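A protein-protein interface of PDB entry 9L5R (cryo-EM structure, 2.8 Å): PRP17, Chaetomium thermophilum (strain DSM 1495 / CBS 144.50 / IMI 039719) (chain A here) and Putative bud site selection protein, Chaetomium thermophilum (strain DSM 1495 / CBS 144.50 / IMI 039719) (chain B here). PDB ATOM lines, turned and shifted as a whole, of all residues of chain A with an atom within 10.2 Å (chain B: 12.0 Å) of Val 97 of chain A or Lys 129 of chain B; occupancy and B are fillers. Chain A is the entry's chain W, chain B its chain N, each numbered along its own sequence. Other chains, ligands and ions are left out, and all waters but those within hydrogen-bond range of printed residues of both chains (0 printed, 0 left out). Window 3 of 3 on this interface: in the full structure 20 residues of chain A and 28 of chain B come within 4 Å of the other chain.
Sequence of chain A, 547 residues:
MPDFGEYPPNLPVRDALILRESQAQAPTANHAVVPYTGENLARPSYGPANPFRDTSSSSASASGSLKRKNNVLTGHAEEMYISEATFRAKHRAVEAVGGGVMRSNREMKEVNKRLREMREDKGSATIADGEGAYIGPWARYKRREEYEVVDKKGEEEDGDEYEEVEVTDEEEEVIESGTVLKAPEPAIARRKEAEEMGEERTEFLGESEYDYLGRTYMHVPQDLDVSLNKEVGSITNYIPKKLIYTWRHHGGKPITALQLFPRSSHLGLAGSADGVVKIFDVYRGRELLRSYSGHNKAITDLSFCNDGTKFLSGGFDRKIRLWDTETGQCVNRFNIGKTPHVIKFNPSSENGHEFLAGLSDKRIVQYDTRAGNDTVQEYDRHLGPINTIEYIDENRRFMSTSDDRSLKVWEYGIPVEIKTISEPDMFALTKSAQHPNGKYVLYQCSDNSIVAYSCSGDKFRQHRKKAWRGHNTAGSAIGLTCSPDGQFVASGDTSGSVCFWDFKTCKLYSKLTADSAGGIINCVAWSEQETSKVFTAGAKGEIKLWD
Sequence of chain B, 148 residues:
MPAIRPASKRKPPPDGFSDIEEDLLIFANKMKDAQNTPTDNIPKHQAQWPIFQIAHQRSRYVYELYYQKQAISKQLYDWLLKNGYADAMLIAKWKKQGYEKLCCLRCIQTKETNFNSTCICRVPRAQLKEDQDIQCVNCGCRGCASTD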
ATOM      1  N   HIS A  91     -18.832   4.957 -15.262  1.00  0.00           N
ATOM      2  CA  HIS A  91     -19.728   4.851 -16.401  1.00  0.00           C
ATOM      3  C   HIS A  91     -20.133   3.409 -16.651  1.00  0.00           C
ATOM      4  O   HIS A  91     -21.296   3.132 -16.943  1.00  0.00           O
ATOM      5  CB  HIS A  91     -19.054   5.441 -17.636  1.00  0.00           C
ATOM      6  CG  HIS A  91     -19.990   5.699 -18.767  1.00  0.00           C
ATOM      7  ND1 HIS A  91     -20.528   4.693 -19.537  1.00  0.00           N
ATOM      8  CD2 HIS A  91     -20.482   6.855 -19.261  1.00  0.00           C
ATOM      9  CE1 HIS A  91     -21.314   5.221 -20.455  1.00  0.00           C
ATOM     10  NE2 HIS A  91     -21.305   6.530 -20.309  1.00  0.00           N
ATOM     11  N   ARG A  92     -19.187   2.479 -16.525  1.00  0.00           N
ATOM     12  CA  ARG A  92     -19.492   1.061 -16.670  1.00  0.00           C
ATOM     13  C   ARG A  92     -20.422   0.564 -15.585  1.00  0.00           C
ATOM     14  O   ARG A  92     -21.302  -0.264 -15.847  1.00  0.00           O
ATOM     15  CB  ARG A  92     -18.204   0.261 -16.657  1.00  0.00           C
ATOM     16  CG  ARG A  92     -18.385  -1.216 -16.838  1.00  0.00           C
ATOM     17  CD  ARG A  92     -18.941  -1.460 -18.186  1.00  0.00           C
ATOM     18  NE  ARG A  92     -18.025  -0.908 -19.161  1.00  0.00           N
ATOM     19  CZ  ARG A  92     -16.956  -1.520 -19.630  1.00  0.00           C
ATOM     20  NH1 ARG A  92     -16.602  -2.719 -19.206  1.00  0.00           N
ATOM     21  NH2 ARG A  92     -16.210  -0.898 -20.532  1.00  0.00           N
ATOM     22  N   ALA A  93     -20.215   1.029 -14.353  1.00  0.00           N
ATOM     23  CA  ALA A  93     -21.057   0.600 -13.247  1.00  0.00           C
ATOM     24  C   ALA A  93     -22.498   1.009 -13.479  1.00  0.00           C
ATOM     25  O   ALA A  93     -23.423   0.246 -13.183  1.00  0.00           O
ATOM     26  CB  ALA A  93     -20.537   1.180 -11.938  1.00  0.00           C
ATOM     27  N   VAL A  94     -22.709   2.203 -14.026  1.00  0.00           N
ATOM     28  CA  VAL A  94     -24.076   2.602 -14.349  1.00  0.00           C
ATOM     29  C   VAL A  94     -24.579   1.879 -15.601  1.00  0.00           C
ATOM     30  O   VAL A  94     -25.732   1.441 -15.654  1.00  0.00           O
ATOM     31  CB  VAL A  94     -24.163   4.130 -14.487  1.00  0.00           C
ATOM     32  CG1 VAL A  94     -25.593   4.560 -14.716  1.00  0.00           C
ATOM     33  CG2 VAL A  94     -23.611   4.793 -13.247  1.00  0.00           C
ATOM     34  N   GLU A  95     -23.724   1.712 -16.611  1.00  0.00           N
ATOM     35  CA  GLU A  95     -24.153   1.349 -17.959  1.00  0.00           C
ATOM     36  C   GLU A  95     -24.321  -0.143 -18.196  1.00  0.00           C
ATOM     37  O   GLU A  95     -25.197  -0.534 -18.974  1.00  0.00           O
ATOM     38  CB  GLU A  95     -23.150   1.889 -18.979  1.00  0.00           C
ATOM     39  CG  GLU A  95     -23.689   1.983 -20.390  1.00  0.00           C
ATOM     40  CD  GLU A  95     -22.625   2.361 -21.385  1.00  0.00           C
ATOM     41  OE1 GLU A  95     -21.430   2.184 -21.066  1.00  0.00           O
ATOM     42  OE2 GLU A  95     -22.977   2.851 -22.476  1.00  0.00           O
ATOM     43  N   ALA A  96     -23.496  -0.988 -17.593  1.00  0.00           N
ATOM     44  CA  ALA A  96     -23.659  -2.418 -17.792  1.00  0.00           C
ATOM     45  C   ALA A  96     -24.899  -2.908 -17.063  1.00  0.00           C
ATOM     46  O   ALA A  96     -25.298  -2.355 -16.037  1.00  0.00           O
ATOM     47  CB  ALA A  96     -22.429  -3.172 -17.297  1.00  0.00           C
ATOM     48  N   VAL A  97     -25.530  -3.944 -17.610  1.00  0.00           N
ATOM     49  CA  VAL A  97     -26.634  -4.564 -16.895  1.00  0.00           C
ATOM     50  C   VAL A  97     -26.074  -5.442 -15.784  1.00  0.00           C
ATOM     51  O   VAL A  97     -24.920  -5.877 -15.817  1.00  0.00           O
ATOM     52  CB  VAL A  97     -27.560  -5.364 -17.827  1.00  0.00           C
ATOM     53  CG1 VAL A  97     -28.076  -4.489 -18.950  1.00  0.00           C
ATOM     54  CG2 VAL A  97     -26.880  -6.604 -18.343  1.00  0.00           C
ATOM     55  N   GLY A  98     -26.906  -5.705 -14.784  1.00  0.00           N
ATOM     56  CA  GLY A  98     -26.434  -6.420 -13.613  1.00  0.00           C
ATOM     57  C   GLY A  98     -25.443  -5.639 -12.779  1.00  0.00           C
ATOM     58  O   GLY A  98     -24.408  -6.190 -12.382  1.00  0.00           O
ATOM     59  N   GLY A  99     -25.723  -4.363 -12.527  1.00  0.00           N
ATOM     60  CA  GLY A  99     -24.823  -3.563 -11.713  1.00  0.00           C
ATOM     61  C   GLY A  99     -24.782  -4.059 -10.277  1.00  0.00           C
ATOM     62  O   GLY A  99     -25.768  -4.576  -9.749  1.00  0.00           O
ATOM     63  N   GLY A 100     -23.627  -3.888  -9.642  1.00  0.00           N
ATOM     64  CA  GLY A 100     -23.416  -4.505  -8.342  1.00  0.00           C
ATOM     65  C   GLY A 100     -23.341  -6.008  -8.510  1.00  0.00           C
ATOM     66  O   GLY A 100     -22.492  -6.524  -9.248  1.00  0.00           O
ATOM     67  N   VAL A 101     -24.256  -6.709  -7.835  1.00  0.00           N
ATOM     68  CA  VAL A 101     -24.486  -8.152  -7.943  1.00  0.00           C
ATOM     69  C   VAL A 101     -23.300  -9.005  -7.511  1.00  0.00           C
ATOM     70  O   VAL A 101     -22.273  -9.092  -8.196  1.00  0.00           O
ATOM     71  CB  VAL A 101     -24.946  -8.559  -9.354  1.00  0.00           C
ATOM     72  CG1 VAL A 101     -25.270 -10.037  -9.367  1.00  0.00           C
ATOM     73  CG2 VAL A 101     -26.192  -7.789  -9.729  1.00  0.00           C
ATOM     74  N   ARG A 103     -21.572 -11.912  -7.714  1.00  0.00           N
ATOM     75  CA  ARG A 103     -21.563 -12.919  -8.758  1.00  0.00           C
ATOM     76  C   ARG A 103     -20.137 -13.248  -9.190  1.00  0.00           C
ATOM     77  O   ARG A 103     -19.383 -12.377  -9.636  1.00  0.00           O
ATOM     78  CB  ARG A 103     -22.443 -12.464  -9.932  1.00  0.00           C
ATOM     79  CG  ARG A 103     -22.542 -13.490 -11.014  1.00  0.00           C
ATOM     80  CD  ARG A 103     -23.494 -13.153 -12.148  1.00  0.00           C
ATOM     81  NE  ARG A 103     -24.908 -13.184 -11.801  1.00  0.00           N
ATOM     82  CZ  ARG A 103     -25.861 -12.773 -12.623  1.00  0.00           C
ATOM     83  NH1 ARG A 103     -25.574 -12.331 -13.836  1.00  0.00           N
ATOM     84  NH2 ARG A 103     -27.129 -12.813 -12.225  1.00  0.00           N
ATOM     85  N   MET A 108     -20.181 -16.585 -13.771  1.00  0.00           N
ATOM     86  CA  MET A 108     -19.885 -15.984 -15.077  1.00  0.00           C
ATOM     87  C   MET A 108     -19.800 -17.048 -16.153  1.00  0.00           C
ATOM     88  O   MET A 108     -20.364 -16.884 -17.240  1.00  0.00           O
ATOM     89  CB  MET A 108     -18.543 -15.241 -15.111  1.00  0.00           C
ATOM     90  CG  MET A 108     -18.177 -13.968 -14.352  1.00  0.00           C
ATOM     91  SD  MET A 108     -19.105 -12.487 -14.745  1.00  0.00           S
ATOM     92  CE  MET A 108     -20.200 -12.376 -13.374  1.00  0.00           C
ATOM     93  N   VAL A 111     -23.221 -18.555 -16.932  1.00  0.00           N
ATOM     94  CA  VAL A 111     -24.087 -17.598 -17.629  1.00  0.00           C
ATOM     95  C   VAL A 111     -23.670 -17.466 -19.089  1.00  0.00           C
ATOM     96  O   VAL A 111     -24.511 -17.498 -20.001  1.00  0.00           O
ATOM     97  CB  VAL A 111     -24.086 -16.234 -16.911  1.00  0.00           C
ATOM     98  CG1 VAL A 111     -24.685 -15.165 -17.798  1.00  0.00           C
ATOM     99  CG2 VAL A 111     -24.896 -16.314 -15.639  1.00  0.00           C
ATOM    100  N   LEU A 115     -25.817 -18.487 -22.497  1.00  0.00           N
ATOM    101  CA  LEU A 115     -25.911 -17.561 -23.623  1.00  0.00           C
ATOM    102  C   LEU A 115     -25.309 -18.147 -24.899  1.00  0.00           C
ATOM    103  O   LEU A 115     -25.820 -17.896 -25.999  1.00  0.00           O
ATOM    104  CB  LEU A 115     -25.235 -16.239 -23.277  1.00  0.00           C
ATOM    105  CG  LEU A 115     -26.178 -15.177 -22.707  1.00  0.00           C
ATOM    106  CD1 LEU A 115     -25.400 -13.997 -22.155  1.00  0.00           C
ATOM    107  CD2 LEU A 115     -27.171 -14.720 -23.760  1.00  0.00           C
ATOM    108  N   TYR A 141     -28.009 -14.470 -32.647  1.00  0.00           N
ATOM    109  CA  TYR A 141     -28.608 -14.851 -31.379  1.00  0.00           C
ATOM    110  C   TYR A 141     -30.055 -15.235 -31.641  1.00  0.00           C
ATOM    111  O   TYR A 141     -30.854 -14.395 -32.067  1.00  0.00           O
ATOM    112  CB  TYR A 141     -28.514 -13.710 -30.372  1.00  0.00           C
ATOM    113  CG  TYR A 141     -27.270 -13.766 -29.524  1.00  0.00           C
ATOM    114  CD1 TYR A 141     -27.216 -14.567 -28.400  1.00  0.00           C
ATOM    115  CD2 TYR A 141     -26.148 -13.023 -29.852  1.00  0.00           C
ATOM    116  CE1 TYR A 141     -26.086 -14.626 -27.623  1.00  0.00           C
ATOM    117  CE2 TYR A 141     -25.008 -13.075 -29.082  1.00  0.00           C
ATOM    118  CZ  TYR A 141     -24.985 -13.880 -27.967  1.00  0.00           C
ATOM    119  OH  TYR A 141     -23.857 -13.945 -27.187  1.00  0.00           O
ATOM    120  N   ARG A 143     -33.710 -15.677 -31.426  1.00  0.00           N
ATOM    121  CA  ARG A 143     -34.834 -15.131 -30.685  1.00  0.00           C
ATOM    122  C   ARG A 143     -36.128 -15.266 -31.477  1.00  0.00           C
ATOM    123  O   ARG A 143     -36.878 -16.225 -31.294  1.00  0.00           O
ATOM    124  CB  ARG A 143     -34.585 -13.667 -30.327  1.00  0.00           C
ATOM    125  CG  ARG A 143     -35.734 -12.987 -29.580  1.00  0.00           C
ATOM    126  CD  ARG A 143     -35.904 -13.494 -28.147  1.00  0.00           C
ATOM    127  NE  ARG A 143     -36.728 -14.693 -28.049  1.00  0.00           N
ATOM    128  CZ  ARG A 143     -36.889 -15.405 -26.941  1.00  0.00           C
ATOM    129  NH1 ARG A 143     -36.282 -15.072 -25.813  1.00  0.00           N
ATOM    130  NH2 ARG A 143     -37.675 -16.476 -26.965  1.00  0.00           N
ATOM    131  N   ILE B 120     -18.984  -2.158 -29.738  1.00  0.00           N
ATOM    132  CA  ILE B 120     -19.893  -2.835 -28.790  1.00  0.00           C
ATOM    133  C   ILE B 120     -19.854  -4.331 -29.062  1.00  0.00           C
ATOM    134  O   ILE B 120     -20.253  -5.084 -28.184  1.00  0.00           O
ATOM    135  CB  ILE B 120     -21.286  -2.215 -28.953  1.00  0.00           C
ATOM    136  CG1 ILE B 120     -22.292  -2.732 -27.925  1.00  0.00           C
ATOM    137  CG2 ILE B 120     -21.780  -2.385 -30.374  1.00  0.00           C
ATOM    138  CD1 ILE B 120     -23.171  -1.658 -27.360  1.00  0.00           C
ATOM    139  N   CYS B 121     -19.314  -4.759 -30.192  1.00  0.00           N
ATOM    140  CA  CYS B 121     -19.367  -6.201 -30.513  1.00  0.00           C
ATOM    141  C   CYS B 121     -18.335  -6.962 -29.698  1.00  0.00           C
ATOM    142  O   CYS B 121     -18.457  -8.176 -29.594  1.00  0.00           O
ATOM    143  CB  CYS B 121     -19.168  -6.419 -31.998  1.00  0.00           C
ATOM    144  SG  CYS B 121     -17.481  -6.252 -32.600  1.00  0.00           S
ATOM    145  N   VAL B 123     -18.002  -6.498 -26.502  1.00  0.00           N
ATOM    146  CA  VAL B 123     -18.499  -6.518 -25.100  1.00  0.00           C
ATOM    147  C   VAL B 123     -19.180  -7.849 -24.841  1.00  0.00           C
ATOM    148  O   VAL B 123     -20.001  -8.244 -25.664  1.00  0.00           O
ATOM    149  CB  VAL B 123     -19.458  -5.350 -24.841  1.00  0.00           C
ATOM    150  CG1 VAL B 123     -20.047  -5.366 -23.443  1.00  0.00           C
ATOM    151  CG2 VAL B 123     -18.772  -4.033 -25.113  1.00  0.00           C
ATOM    152  N   PRO B 124     -18.840  -8.569 -23.753  1.00  0.00           N
ATOM    153  CA  PRO B 124     -19.532  -9.802 -23.418  1.00  0.00           C
ATOM    154  C   PRO B 124     -21.046  -9.587 -23.376  1.00  0.00           C
ATOM    155  O   PRO B 124     -21.468  -8.740 -22.649  1.00  0.00           O
ATOM    156  CB  PRO B 124     -18.987 -10.073 -22.025  1.00  0.00           C
ATOM    157  CG  PRO B 124     -17.589  -9.535 -22.060  1.00  0.00           C
ATOM    158  CD  PRO B 124     -17.733  -8.260 -22.851  1.00  0.00           C
ATOM    159  N   ARG B 125     -21.813 -10.329 -24.175  1.00  0.00           N
ATOM    160  CA  ARG B 125     -23.264 -10.198 -24.217  1.00  0.00           C
ATOM    161  C   ARG B 125     -23.927 -10.423 -22.871  1.00  0.00           C
ATOM    162  O   ARG B 125     -25.128 -10.172 -22.745  1.00  0.00           O
ATOM    163  CB  ARG B 125     -23.853 -11.144 -25.258  1.00  0.00           C
ATOM    164  CG  ARG B 125     -23.384 -10.772 -26.639  1.00  0.00           C
ATOM    165  CD  ARG B 125     -24.014  -9.454 -27.017  1.00  0.00           C
ATOM    166  NE  ARG B 125     -23.719  -9.025 -28.376  1.00  0.00           N
ATOM    167  CZ  ARG B 125     -22.687  -8.260 -28.707  1.00  0.00           C
ATOM    168  NH1 ARG B 125     -21.776  -7.906 -27.815  1.00  0.00           N
ATOM    169  NH2 ARG B 125     -22.566  -7.843 -29.960  1.00  0.00           N
ATOM    170  N   ALA B 126     -23.185 -10.870 -21.865  1.00  0.00           N
ATOM    171  CA  ALA B 126     -23.752 -10.981 -20.532  1.00  0.00           C
ATOM    172  C   ALA B 126     -23.995  -9.623 -19.899  1.00  0.00           C
ATOM    173  O   ALA B 126     -24.784  -9.528 -18.955  1.00  0.00           O
ATOM    174  CB  ALA B 126     -22.834 -11.814 -19.642  1.00  0.00           C
ATOM    175  N   GLN B 127     -23.340  -8.574 -20.391  1.00  0.00           N
ATOM    176  CA  GLN B 127     -23.463  -7.236 -19.836  1.00  0.00           C
ATOM    177  C   GLN B 127     -24.342  -6.332 -20.675  1.00  0.00           C
ATOM    178  O   GLN B 127     -24.369  -5.124 -20.438  1.00  0.00           O
ATOM    179  CB  GLN B 127     -22.090  -6.597 -19.678  1.00  0.00           C
ATOM    180  CG  GLN B 127     -21.039  -7.556 -19.244  1.00  0.00           C
ATOM    181  CD  GLN B 127     -19.728  -6.882 -18.994  1.00  0.00           C
ATOM    182  OE1 GLN B 127     -19.535  -5.724 -19.351  1.00  0.00           O
ATOM    183  NE2 GLN B 127     -18.811  -7.602 -18.367  1.00  0.00           N
ATOM    184  N   LEU B 128     -25.057  -6.876 -21.641  1.00  0.00           N
ATOM    185  CA  LEU B 128     -25.918  -6.079 -22.494  1.00  0.00           C
ATOM    186  C   LEU B 128     -27.374  -6.452 -22.248  1.00  0.00           C
ATOM    187  O   LEU B 128     -27.683  -7.430 -21.563  1.00  0.00           O
ATOM    188  CB  LEU B 128     -25.528  -6.265 -23.963  1.00  0.00           C
ATOM    189  CG  LEU B 128     -24.131  -5.744 -24.322  1.00  0.00           C
ATOM    190  CD1 LEU B 128     -23.795  -6.046 -25.750  1.00  0.00           C
ATOM    191  CD2 LEU B 128     -24.020  -4.256 -24.078  1.00  0.00           C
ATOM    192  N   LYS B 129     -28.273  -5.634 -22.791  1.00  0.00           N
ATOM    193  CA  LYS B 129     -29.700  -5.868 -22.616  1.00  0.00           C
ATOM    194  C   LYS B 129     -30.117  -7.155 -23.311  1.00  0.00           C
ATOM    195  O   LYS B 129     -29.510  -7.585 -24.292  1.00  0.00           O
ATOM    196  CB  LYS B 129     -30.512  -4.701 -23.176  1.00  0.00           C
ATOM    197  CG  LYS B 129     -30.171  -3.350 -22.594  1.00  0.00           C
ATOM    198  CD  LYS B 129     -30.764  -3.168 -21.215  1.00  0.00           C
ATOM    199  CE  LYS B 129     -30.506  -1.763 -20.689  1.00  0.00           C
ATOM    200  NZ  LYS B 129     -29.055  -1.491 -20.477  1.00  0.00           N
ATOM    201  N   GLU B 130     -31.151  -7.790 -22.775  1.00  0.00           N
ATOM    202  CA  GLU B 130     -31.689  -8.973 -23.423  1.00  0.00           C
ATOM    203  C   GLU B 130     -32.453  -8.564 -24.672  1.00  0.00           C
ATOM    204  O   GLU B 130     -33.133  -7.533 -24.690  1.00  0.00           O
ATOM    205  CB  GLU B 130     -32.594  -9.743 -22.463  1.00  0.00           C
ATOM    206  CG  GLU B 130     -31.915 -10.127 -21.163  1.00  0.00           C
ATOM    207  CD  GLU B 130     -30.721 -11.032 -21.373  1.00  0.00           C
ATOM    208  OE1 GLU B 130     -30.790 -11.919 -22.251  1.00  0.00           O
ATOM    209  OE2 GLU B 130     -29.710 -10.857 -20.664  1.00  0.00           O
ATOM    210  N   ASP B 131     -32.312  -9.373 -25.726  1.00  0.00           N
ATOM    211  CA  ASP B 131     -32.877  -9.109 -27.053  1.00  0.00           C
ATOM    212  C   ASP B 131     -32.396  -7.777 -27.625  1.00  0.00           C
ATOM    213  O   ASP B 131     -33.099  -7.136 -28.407  1.00  0.00           O
ATOM    214  CB  ASP B 131     -34.410  -9.172 -27.044  1.00  0.00           C
ATOM    215  CG  ASP B 131     -34.933 -10.448 -26.420  1.00  0.00           C
ATOM    216  OD1 ASP B 131     -34.149 -11.411 -26.300  1.00  0.00           O
ATOM    217  OD2 ASP B 131     -36.128 -10.490 -26.057  1.00  0.00           O
ATOM    218  N   GLN B 132     -31.197  -7.351 -27.230  1.00  0.00           N
ATOM    219  CA  GLN B 132     -30.544  -6.175 -27.799  1.00  0.00           C
ATOM    220  C   GLN B 132     -29.653  -6.674 -28.922  1.00  0.00           C
ATOM    221  O   GLN B 132     -28.508  -7.070 -28.707  1.00  0.00           O
ATOM    222  CB  GLN B 132     -29.752  -5.422 -26.739  1.00  0.00           C
ATOM    223  CG  GLN B 132     -29.004  -4.206 -27.248  1.00  0.00           C
ATOM    224  CD  GLN B 132     -28.008  -3.686 -26.239  1.00  0.00           C
ATOM    225  OE1 GLN B 132     -27.867  -4.238 -25.155  1.00  0.00           O
ATOM    226  NE2 GLN B 132     -27.313  -2.614 -26.589  1.00  0.00           N
ATOM    227  N   ASP B 133     -30.191  -6.672 -30.135  1.00  0.00           N
ATOM    228  CA  ASP B 133     -29.490  -7.239 -31.279  1.00  0.00           C
ATOM    229  C   ASP B 133     -28.475  -6.228 -31.795  1.00  0.00           C
ATOM    230  O   ASP B 133     -28.834  -5.250 -32.456  1.00  0.00           O
ATOM    231  CB  ASP B 133     -30.478  -7.634 -32.368  1.00  0.00           C
ATOM    232  CG  ASP B 133     -29.790  -8.133 -33.616  1.00  0.00           C
ATOM    233  OD1 ASP B 133     -29.197  -9.231 -33.570  1.00  0.00           O
ATOM    234  OD2 ASP B 133     -29.841  -7.426 -34.644  1.00  0.00           O
ATOM    235  N   ILE B 134     -27.209  -6.464 -31.490  1.00  0.00           N
ATOM    236  CA  ILE B 134     -26.104  -5.671 -32.001  1.00  0.00           C
ATOM    237  C   ILE B 134     -25.664  -6.231 -33.342  1.00  0.00           C
ATOM    238  O   ILE B 134     -25.489  -7.445 -33.492  1.00  0.00           O
ATOM    239  CB  ILE B 134     -24.935  -5.653 -31.004  1.00  0.00           C
ATOM    240  CG1 ILE B 134     -25.379  -5.059 -29.667  1.00  0.00           C
ATOM    241  CG2 ILE B 134     -23.724  -4.977 -31.592  1.00  0.00           C
ATOM    242  CD1 ILE B 134     -25.853  -3.634 -29.775  1.00  0.00           C
ATOM    243  N   GLN B 135     -25.416  -5.346 -34.308  1.00  0.00           N
ATOM    244  CA  GLN B 135     -24.778  -5.713 -35.596  1.00  0.00           C
ATOM    245  C   GLN B 135     -23.879  -4.510 -35.869  1.00  0.00           C
ATOM    246  O   GLN B 135     -24.392  -3.545 -36.424  1.00  0.00           O
ATOM    247  CB  GLN B 135     -25.809  -5.978 -36.680  1.00  0.00           C
ATOM    248  CG  GLN B 135     -25.847  -7.431 -37.104  1.00  0.00           C
ATOM    249  CD  GLN B 135     -26.298  -7.603 -38.531  1.00  0.00           C
ATOM    250  OE1 GLN B 135     -27.350  -7.116 -38.931  1.00  0.00           O
ATOM    251  NE2 GLN B 135     -25.505  -8.323 -39.305  1.00  0.00           N
ATOM    252  N   ARG B 142     -22.109  -9.790 -34.573  1.00  0.00           N
ATOM    253  CA  ARG B 142     -23.203  -9.822 -33.590  1.00  0.00           C
ATOM    254  C   ARG B 142     -22.652 -10.149 -32.207  1.00  0.00           C
ATOM    255  O   ARG B 142     -23.454 -10.209 -31.284  1.00  0.00           O
ATOM    256  CB  ARG B 142     -24.217 -10.846 -34.082  1.00  0.00           C
ATOM    257  CG  ARG B 142     -24.588 -10.688 -35.545  1.00  0.00           C
ATOM    258  CD  ARG B 142     -25.696 -11.658 -35.857  1.00  0.00           C
ATOM    259  NE  ARG B 142     -26.352 -11.386 -37.119  1.00  0.00           N
ATOM    260  CZ  ARG B 142     -27.510 -10.756 -37.230  1.00  0.00           C
ATOM    261  NH1 ARG B 142     -28.135 -10.321 -36.151  1.00  0.00           N
ATOM    262  NH2 ARG B 142     -28.035 -10.551 -38.422  1.00  0.00           N
ATOM    263  N   GLY B 143     -21.343 -10.338 -32.072  1.00  0.00           N
ATOM    264  CA  GLY B 143     -20.726 -10.722 -30.791  1.00  0.00           C
ATOM    265  C   GLY B 143     -19.422 -11.433 -31.031  1.00  0.00           C
ATOM    266  O   GLY B 143     -19.446 -12.517 -31.593  1.00  0.00           O
ATOM    267  N   ASP B 148     -18.480 -15.091 -25.506  1.00  0.00           N
ATOM    268  CA  ASP B 148     -19.589 -15.246 -26.442  1.00  0.00           C
ATOM    269  C   ASP B 148     -19.325 -16.334 -27.477  1.00  0.00           C
ATOM    270  O   ASP B 148     -20.116 -16.526 -28.396  1.00  0.00           O
ATOM    271  CB  ASP B 148     -19.869 -13.932 -27.166  1.00  0.00           C
ATOM    272  CG  ASP B 148     -20.191 -12.801 -26.221  1.00  0.00           C
ATOM    273  OD1 ASP B 148     -20.423 -13.061 -25.025  1.00  0.00           O
ATOM    274  OD2 ASP B 148     -20.206 -11.643 -26.681  1.00  0.00           O
ATOM    275  OXT ASP B 148     -18.323 -17.042 -27.441  1.00  0.00           O
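NH1 of Arg 125 of chain B lies within hydrogen-bond range of O of Ile 120 of chain B, 3.2 Å away.
O of Val 123 of chain B is in hydrogen-bond range of NH1 of Arg 125 of chain B (2.8 Å).
NH2 of Arg 125 of chain B is in hydrogen-bond range of O of Arg 142 of chain B (2.9 Å).
The side-chain carboxylate (OD1) of Asp 148 of chain B sits at hydrogen-bond distance from the backbone NH (N) of Arg 125 of chain B (3.2 Å).
N of Lys 129 of chain B lies within hydrogen-bond range of OE1 of Gln 132 of chain B, at 2.8 Å.
NH2 of Arg 142 of chain B sits close to NE2 of Gln 135 of chain B (3.5 Å).
No residue of chain B comes within 4 Å of Gly 98 of chain A.
No residue of chain B comes within 4 Å of Gly 99 of chain A.
Of the printed residues of chain B, Leu 115 of chain A touches Arg 125 and Ala 126.
Of the printed residues of chain B, Tyr 141 of chain A touches Arg 125, Arg 142 and Asp 148.
Val 123 of chain B touches none of the printed residues of chain A.
Printed residues of chain A within 4 Å of Gln 127 of chain B: Ala 96 and Val 97.
Of chain A, only Val 97 (3.4 Å) comes within 4 Å of Leu 128 of chain B.
Of chain A, only Val 97 (3.5 Å) comes within 4 Å of Lys 129 of chain B.
No residue of chain A comes within 4 Å of Glu 130 of chain B.
Printed residues of chain A within 4 Å of Asp 131 of chain B: Arg 143.
Of the printed residues of chain A, Asp 148 of chain B touches Tyr 141 (3.96 Å).
The nearest residue of chain A that does not touch Lys 129 of chain B is Glu 95 of chain A (4.2 Å).
The nearest printed residue of chain B that does not touch Arg 143 of chain A is Glu 130 of chain B (6.9 Å).
O of Gln 127 of chain B sits at hydrogen-bond distance from N of Val 97 of chain A (3.3 Å).
Of the 17 printed residues of chain A, 5 touch a printed residue of chain B.
Printed residues of chain B that touch a printed residue of chain A: Arg 125, Ala 126, Gln 127, Leu 128, Lys 129, Asp 131, Arg 142 and Asp 148.
Among the printed residues, 11 pairs touch across the chains.
Among the printed residues, no Asp or Glu carboxylate lies within 4 Å of a Lys or Arg side-chain nitrogen of the other chain.
Gln 127 of chain B touches Ala 96 of chain A (O to CA, 3.9 Å).
Val 97 of chain A touches Ala 126 of chain B (CG2 to O, 3.6 Å).
Leu 128 of chain B touches Val 97 of chain A.
Val 97 of chain A touches Lys 129 of chain B (CG1 to NZ, 3.5 Å).
O of Arg 125 of chain B touches CD1 of Leu 115 of chain A, at 3.9 Å.
CD1 of Leu 115 of chain A touches CA of Ala 126 of chain B (3.8 Å).
Arg 125 of chain B touches Tyr 141 of chain A (CG to OH, 3.3 Å).
Tyr 141 of chain A touches Arg 142 of chain B.
Asp 148 of chain B touches Tyr 141 of chain A (CG to OH, 3.96 Å).
Arg 143 of chain A touches Asp 131 of chain B (CD to OD1, 3.3 Å).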
